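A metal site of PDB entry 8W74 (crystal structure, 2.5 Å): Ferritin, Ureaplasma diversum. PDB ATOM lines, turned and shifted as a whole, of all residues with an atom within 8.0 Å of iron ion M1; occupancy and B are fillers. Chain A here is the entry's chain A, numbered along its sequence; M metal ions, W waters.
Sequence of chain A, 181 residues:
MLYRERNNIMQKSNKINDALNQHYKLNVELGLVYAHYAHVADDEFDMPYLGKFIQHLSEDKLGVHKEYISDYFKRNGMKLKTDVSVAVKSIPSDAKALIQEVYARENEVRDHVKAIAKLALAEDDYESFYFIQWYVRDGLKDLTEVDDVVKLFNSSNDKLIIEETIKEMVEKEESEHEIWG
NZ of Lys 141 is in salt-bridge range of OD1 of Asp 138 (3.6 Å). The side-chain carboxylate of Asp 138 is in salt-bridge range of the guanidinium group of Arg 137, at 3.1 Å. The side-chain carboxylate (OD1) of Asp 142 is in salt-bridge range of the side-chain amino group (NZ) of Lys 141 (2.8 Å). NZ of Lys 61 sits close to OD2 of Asp 142, at 2.8 Å. ND1 of His 65 lies within hydrogen-bond range of OD1 of Asn 27 (3.1 Å). O of His 65 is in hydrogen-bond range of OH of Tyr 135 (2.8 Å). The side-chain carboxylate (OE1) of Glu 145 is in salt-bridge range of the side-chain amino group (NZ) of Lys 141 (3.8 Å).
Residues that only touch iron ion M1: Lys 141. Of the 19 residues printed, 5 come within 4 Å of iron ion M1. The nearest printed residue that does not touch iron ion M1 is Lys 61 (4.4 Å).
Iron ion M1 is bound by OD2 of Asp 138, OD2 of Asp 60, OD2 of Asp 142, NE2 of His 65 and water W1. Iron ion M1 has five donor atoms within binding distance. Slightly farther from iron ion M1 lies OD1 of Asp 142 (2.7 Å).
Water W1 lies within hydrogen-bond range of the side-chain carboxylate of Asp 60, the side-chain carboxylate of Asp 138 and the side-chain amino group of Lys 141.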
ATOM      1  N   ASN A  27     -18.389 -15.073  36.371  1.00  0.00           N
ATOM      2  CA  ASN A  27     -18.183 -13.696  35.940  1.00  0.00           C
ATOM      3  C   ASN A  27     -17.683 -12.804  37.084  1.00  0.00           C
ATOM      4  O   ASN A  27     -16.868 -11.906  36.842  1.00  0.00           O
ATOM      5  CB  ASN A  27     -19.465 -13.132  35.318  1.00  0.00           C
ATOM      6  CG  ASN A  27     -19.620 -13.535  33.860  1.00  0.00           C
ATOM      7  OD1 ASN A  27     -18.971 -12.983  32.981  1.00  0.00           O
ATOM      8  ND2 ASN A  27     -20.456 -14.539  33.604  1.00  0.00           N
ATOM      9  N   HIS A  56     -11.457  -2.489  31.667  1.00  0.00           N
ATOM     10  CA  HIS A  56     -12.796  -2.447  31.089  1.00  0.00           C
ATOM     11  C   HIS A  56     -13.406  -3.832  31.033  1.00  0.00           C
ATOM     12  O   HIS A  56     -14.601  -4.006  31.312  1.00  0.00           O
ATOM     13  CB  HIS A  56     -12.777  -1.833  29.690  1.00  0.00           C
ATOM     14  CG  HIS A  56     -12.453  -0.370  29.674  1.00  0.00           C
ATOM     15  ND1 HIS A  56     -12.338   0.376  30.831  1.00  0.00           N
ATOM     16  CD2 HIS A  56     -12.244   0.485  28.653  1.00  0.00           C
ATOM     17  CE1 HIS A  56     -12.051   1.626  30.513  1.00  0.00           C
ATOM     18  NE2 HIS A  56     -11.985   1.719  29.202  1.00  0.00           N
ATOM     19  N   LEU A  57     -12.609  -4.841  30.671  1.00  0.00           N
ATOM     20  CA  LEU A  57     -13.104  -6.213  30.686  1.00  0.00           C
ATOM     21  C   LEU A  57     -13.495  -6.637  32.099  1.00  0.00           C
ATOM     22  O   LEU A  57     -14.498  -7.336  32.287  1.00  0.00           O
ATOM     23  CB  LEU A  57     -12.062  -7.165  30.096  1.00  0.00           C
ATOM     24  CG  LEU A  57     -12.545  -8.539  29.636  1.00  0.00           C
ATOM     25  CD1 LEU A  57     -13.671  -8.440  28.625  1.00  0.00           C
ATOM     26  CD2 LEU A  57     -11.392  -9.352  29.070  1.00  0.00           C
ATOM     27  N   GLU A  59     -14.687  -4.699  34.524  1.00  0.00           N
ATOM     28  CA  GLU A  59     -15.951  -4.047  34.826  1.00  0.00           C
ATOM     29  C   GLU A  59     -17.109  -4.604  34.004  1.00  0.00           C
ATOM     30  O   GLU A  59     -18.251  -4.606  34.472  1.00  0.00           O
ATOM     31  CB  GLU A  59     -15.811  -2.553  34.614  1.00  0.00           C
ATOM     32  CG  GLU A  59     -14.984  -1.891  35.705  1.00  0.00           C
ATOM     33  CD  GLU A  59     -14.264  -0.655  35.236  1.00  0.00           C
ATOM     34  OE1 GLU A  59     -13.374  -0.207  35.985  1.00  0.00           O
ATOM     35  OE2 GLU A  59     -14.595  -0.136  34.144  1.00  0.00           O
ATOM     36  N   ASP A  60     -16.846  -5.068  32.795  1.00  0.00           N
ATOM     37  CA  ASP A  60     -17.871  -5.780  32.042  1.00  0.00           C
ATOM     38  C   ASP A  60     -18.304  -7.051  32.773  1.00  0.00           C
ATOM     39  O   ASP A  60     -19.504  -7.262  33.011  1.00  0.00           O
ATOM     40  CB  ASP A  60     -17.334  -6.087  30.635  1.00  0.00           C
ATOM     41  CG  ASP A  60     -18.366  -6.724  29.745  1.00  0.00           C
ATOM     42  OD1 ASP A  60     -19.543  -6.291  29.767  1.00  0.00           O
ATOM     43  OD2 ASP A  60     -17.987  -7.667  29.008  1.00  0.00           O
ATOM     44  N   LYS A  61     -17.342  -7.894  33.176  1.00  0.00           N
ATOM     45  CA  LYS A  61     -17.683  -9.144  33.851  1.00  0.00           C
ATOM     46  C   LYS A  61     -18.396  -8.893  35.178  1.00  0.00           C
ATOM     47  O   LYS A  61     -19.362  -9.600  35.514  1.00  0.00           O
ATOM     48  CB  LYS A  61     -16.430  -9.987  34.102  1.00  0.00           C
ATOM     49  CG  LYS A  61     -15.616 -10.385  32.860  1.00  0.00           C
ATOM     50  CD  LYS A  61     -16.442 -11.177  31.851  1.00  0.00           C
ATOM     51  CE  LYS A  61     -15.587 -11.656  30.680  1.00  0.00           C
ATOM     52  NZ  LYS A  61     -16.412 -12.135  29.518  1.00  0.00           N
ATOM     53  N   VAL A  64     -22.680  -5.958  33.828  1.00  0.00           N
ATOM     54  CA  VAL A  64     -23.865  -6.489  33.170  1.00  0.00           C
ATOM     55  C   VAL A  64     -23.840  -8.010  33.104  1.00  0.00           C
ATOM     56  O   VAL A  64     -24.902  -8.651  33.195  1.00  0.00           O
ATOM     57  CB  VAL A  64     -24.038  -5.876  31.775  1.00  0.00           C
ATOM     58  CG1 VAL A  64     -24.290  -4.402  31.925  1.00  0.00           C
ATOM     59  CG2 VAL A  64     -22.830  -6.161  30.874  1.00  0.00           C
ATOM     60  N   HIS A  65     -22.691  -8.635  33.014  1.00  0.00           N
ATOM     61  CA  HIS A  65     -22.645 -10.064  32.944  1.00  0.00           C
ATOM     62  C   HIS A  65     -23.252 -10.703  34.171  1.00  0.00           C
ATOM     63  O   HIS A  65     -23.855 -11.743  34.080  1.00  0.00           O
ATOM     64  CB  HIS A  65     -21.230 -10.516  32.796  1.00  0.00           C
ATOM     65  CG  HIS A  65     -20.704 -10.470  31.404  1.00  0.00           C
ATOM     66  ND1 HIS A  65     -20.533 -11.592  30.643  1.00  0.00           N
ATOM     67  CD2 HIS A  65     -20.256  -9.437  30.661  1.00  0.00           C
ATOM     68  CE1 HIS A  65     -20.032 -11.263  29.476  1.00  0.00           C
ATOM     69  NE2 HIS A  65     -19.856  -9.954  29.460  1.00  0.00           N
ATOM     70  N   GLU A 106     -11.488 -16.397  28.323  1.00  0.00           N
ATOM     71  CA  GLU A 106     -12.630 -16.035  27.474  1.00  0.00           C
ATOM     72  C   GLU A 106     -13.050 -17.204  26.591  1.00  0.00           C
ATOM     73  O   GLU A 106     -14.252 -17.417  26.347  1.00  0.00           O
ATOM     74  CB  GLU A 106     -12.314 -14.827  26.596  1.00  0.00           C
ATOM     75  CG  GLU A 106     -12.099 -13.542  27.345  1.00  0.00           C
ATOM     76  CD  GLU A 106     -13.263 -13.202  28.240  1.00  0.00           C
ATOM     77  OE1 GLU A 106     -14.403 -13.185  27.751  1.00  0.00           O
ATOM     78  OE2 GLU A 106     -13.016 -12.948  29.429  1.00  0.00           O
ATOM     79  N   VAL A 109     -15.234 -19.201  28.637  1.00  0.00           N
ATOM     80  CA  VAL A 109     -16.557 -18.584  28.710  1.00  0.00           C
ATOM     81  C   VAL A 109     -17.448 -19.116  27.596  1.00  0.00           C
ATOM     82  O   VAL A 109     -18.590 -19.527  27.831  1.00  0.00           O
ATOM     83  CB  VAL A 109     -16.448 -17.053  28.668  1.00  0.00           C
ATOM     84  CG1 VAL A 109     -17.825 -16.428  28.410  1.00  0.00           C
ATOM     85  CG2 VAL A 109     -15.822 -16.521  29.974  1.00  0.00           C
ATOM     86  N   TRP A 134     -27.781 -13.505  24.557  1.00  0.00           N
ATOM     87  CA  TRP A 134     -26.876 -12.399  24.855  1.00  0.00           C
ATOM     88  C   TRP A 134     -25.485 -12.912  25.172  1.00  0.00           C
ATOM     89  O   TRP A 134     -24.484 -12.412  24.644  1.00  0.00           O
ATOM     90  CB  TRP A 134     -27.419 -11.579  26.031  1.00  0.00           C
ATOM     91  CG  TRP A 134     -26.668 -10.311  26.254  1.00  0.00           C
ATOM     92  CD1 TRP A 134     -26.949  -9.107  25.708  1.00  0.00           C
ATOM     93  CD2 TRP A 134     -25.515 -10.130  27.090  1.00  0.00           C
ATOM     94  NE1 TRP A 134     -26.042  -8.164  26.146  1.00  0.00           N
ATOM     95  CE2 TRP A 134     -25.156  -8.765  26.998  1.00  0.00           C
ATOM     96  CE3 TRP A 134     -24.752 -10.980  27.901  1.00  0.00           C
ATOM     97  CZ2 TRP A 134     -24.051  -8.223  27.674  1.00  0.00           C
ATOM     98  CZ3 TRP A 134     -23.654 -10.431  28.591  1.00  0.00           C
ATOM     99  CH2 TRP A 134     -23.321  -9.066  28.472  1.00  0.00           C
ATOM    100  N   TYR A 135     -25.402 -13.941  26.027  1.00  0.00           N
ATOM    101  CA  TYR A 135     -24.134 -14.530  26.425  1.00  0.00           C
ATOM    102  C   TYR A 135     -23.497 -15.347  25.314  1.00  0.00           C
ATOM    103  O   TYR A 135     -22.268 -15.376  25.204  1.00  0.00           O
ATOM    104  CB  TYR A 135     -24.339 -15.389  27.673  1.00  0.00           C
ATOM    105  CG  TYR A 135     -24.742 -14.554  28.855  1.00  0.00           C
ATOM    106  CD1 TYR A 135     -26.056 -14.136  29.019  1.00  0.00           C
ATOM    107  CD2 TYR A 135     -23.791 -14.148  29.793  1.00  0.00           C
ATOM    108  CE1 TYR A 135     -26.421 -13.347  30.109  1.00  0.00           C
ATOM    109  CE2 TYR A 135     -24.132 -13.361  30.882  1.00  0.00           C
ATOM    110  CZ  TYR A 135     -25.459 -12.960  31.040  1.00  0.00           C
ATOM    111  OH  TYR A 135     -25.825 -12.172  32.116  1.00  0.00           O
ATOM    112  N   ARG A 137     -23.733 -14.499  22.184  1.00  0.00           N
ATOM    113  CA  ARG A 137     -23.160 -13.467  21.334  1.00  0.00           C
ATOM    114  C   ARG A 137     -21.956 -12.815  21.994  1.00  0.00           C
ATOM    115  O   ARG A 137     -20.913 -12.611  21.347  1.00  0.00           O
ATOM    116  CB  ARG A 137     -24.221 -12.412  21.000  1.00  0.00           C
ATOM    117  CG  ARG A 137     -23.683 -11.232  20.182  1.00  0.00           C
ATOM    118  CD  ARG A 137     -24.386  -9.894  20.477  1.00  0.00           C
ATOM    119  NE  ARG A 137     -24.582  -9.594  21.901  1.00  0.00           N
ATOM    120  CZ  ARG A 137     -23.628  -9.181  22.739  1.00  0.00           C
ATOM    121  NH1 ARG A 137     -22.380  -9.032  22.324  1.00  0.00           N
ATOM    122  NH2 ARG A 137     -23.923  -8.951  24.009  1.00  0.00           N
ATOM    123  N   ASP A 138     -22.055 -12.485  23.277  1.00  0.00           N
ATOM    124  CA  ASP A 138     -20.965 -11.785  23.963  1.00  0.00           C
ATOM    125  C   ASP A 138     -19.730 -12.648  24.124  1.00  0.00           C
ATOM    126  O   ASP A 138     -18.626 -12.105  24.255  1.00  0.00           O
ATOM    127  CB  ASP A 138     -21.432 -11.292  25.324  1.00  0.00           C
ATOM    128  CG  ASP A 138     -20.768 -10.012  25.735  1.00  0.00           C
ATOM    129  OD1 ASP A 138     -21.046  -8.962  25.110  1.00  0.00           O
ATOM    130  OD2 ASP A 138     -19.961 -10.043  26.691  1.00  0.00           O
ATOM    131  N   GLY A 139     -19.886 -13.981  24.147  1.00  0.00           N
ATOM    132  CA  GLY A 139     -18.726 -14.855  24.235  1.00  0.00           C
ATOM    133  C   GLY A 139     -17.767 -14.644  23.082  1.00  0.00           C
ATOM    134  O   GLY A 139     -16.547 -14.550  23.279  1.00  0.00           O
ATOM    135  N   LYS A 141     -17.877 -11.890  20.888  1.00  0.00           N
ATOM    136  CA  LYS A 141     -17.473 -10.475  20.962  1.00  0.00           C
ATOM    137  C   LYS A 141     -16.281 -10.281  21.880  1.00  0.00           C
ATOM    138  O   LYS A 141     -15.244  -9.755  21.469  1.00  0.00           O
ATOM    139  CB  LYS A 141     -18.650  -9.624  21.435  1.00  0.00           C
ATOM    140  CG  LYS A 141     -18.548  -8.140  21.063  1.00  0.00           C
ATOM    141  CD  LYS A 141     -18.789  -7.216  22.261  1.00  0.00           C
ATOM    142  CE  LYS A 141     -17.919  -7.623  23.439  1.00  0.00           C
ATOM    143  NZ  LYS A 141     -18.116  -6.838  24.697  1.00  0.00           N
ATOM    144  N   ASP A 142     -16.417 -10.685  23.150  1.00  0.00           N
ATOM    145  CA  ASP A 142     -15.328 -10.523  24.111  1.00  0.00           C
ATOM    146  C   ASP A 142     -14.073 -11.228  23.634  1.00  0.00           C
ATOM    147  O   ASP A 142     -12.969 -10.685  23.751  1.00  0.00           O
ATOM    148  CB  ASP A 142     -15.741 -11.052  25.479  1.00  0.00           C
ATOM    149  CG  ASP A 142     -16.552 -10.059  26.274  1.00  0.00           C
ATOM    150  OD1 ASP A 142     -16.641  -8.890  25.846  1.00  0.00           O
ATOM    151  OD2 ASP A 142     -17.102 -10.430  27.346  1.00  0.00           O
ATOM    152  N   LEU A 143     -14.219 -12.451  23.114  1.00  0.00           N
ATOM    153  CA  LEU A 143     -13.044 -13.175  22.621  1.00  0.00           C
ATOM    154  C   LEU A 143     -12.363 -12.415  21.478  1.00  0.00           C
ATOM    155  O   LEU A 143     -11.131 -12.361  21.414  1.00  0.00           O
ATOM    156  CB  LEU A 143     -13.439 -14.582  22.171  1.00  0.00           C
ATOM    157  CG  LEU A 143     -12.232 -15.465  21.825  1.00  0.00           C
ATOM    158  CD1 LEU A 143     -11.801 -16.263  23.028  1.00  0.00           C
ATOM    159  CD2 LEU A 143     -12.555 -16.390  20.658  1.00  0.00           C
ATOM    160  N   GLU A 145     -12.412  -9.092  20.847  1.00  0.00           N
ATOM    161  CA  GLU A 145     -11.716  -7.936  21.388  1.00  0.00           C
ATOM    162  C   GLU A 145     -10.388  -8.346  22.010  1.00  0.00           C
ATOM    163  O   GLU A 145      -9.364  -7.714  21.773  1.00  0.00           O
ATOM    164  CB  GLU A 145     -12.597  -7.213  22.396  1.00  0.00           C
ATOM    165  CG  GLU A 145     -13.827  -6.537  21.774  1.00  0.00           C
ATOM    166  CD  GLU A 145     -14.694  -5.781  22.786  1.00  0.00           C
ATOM    167  OE1 GLU A 145     -14.460  -5.912  24.018  1.00  0.00           O
ATOM    168  OE2 GLU A 145     -15.613  -5.057  22.350  1.00  0.00           O
HETATM  169 FE    FE M   1     -18.757  -8.919  27.574  1.00  0.00          FE
HETATM  170 FE    FE M   2     -16.946  -3.671  25.952  1.00  0.00          FE
HETATM  171  O   HOH W   1     -20.032  -6.924  27.011  1.00  0.00           O
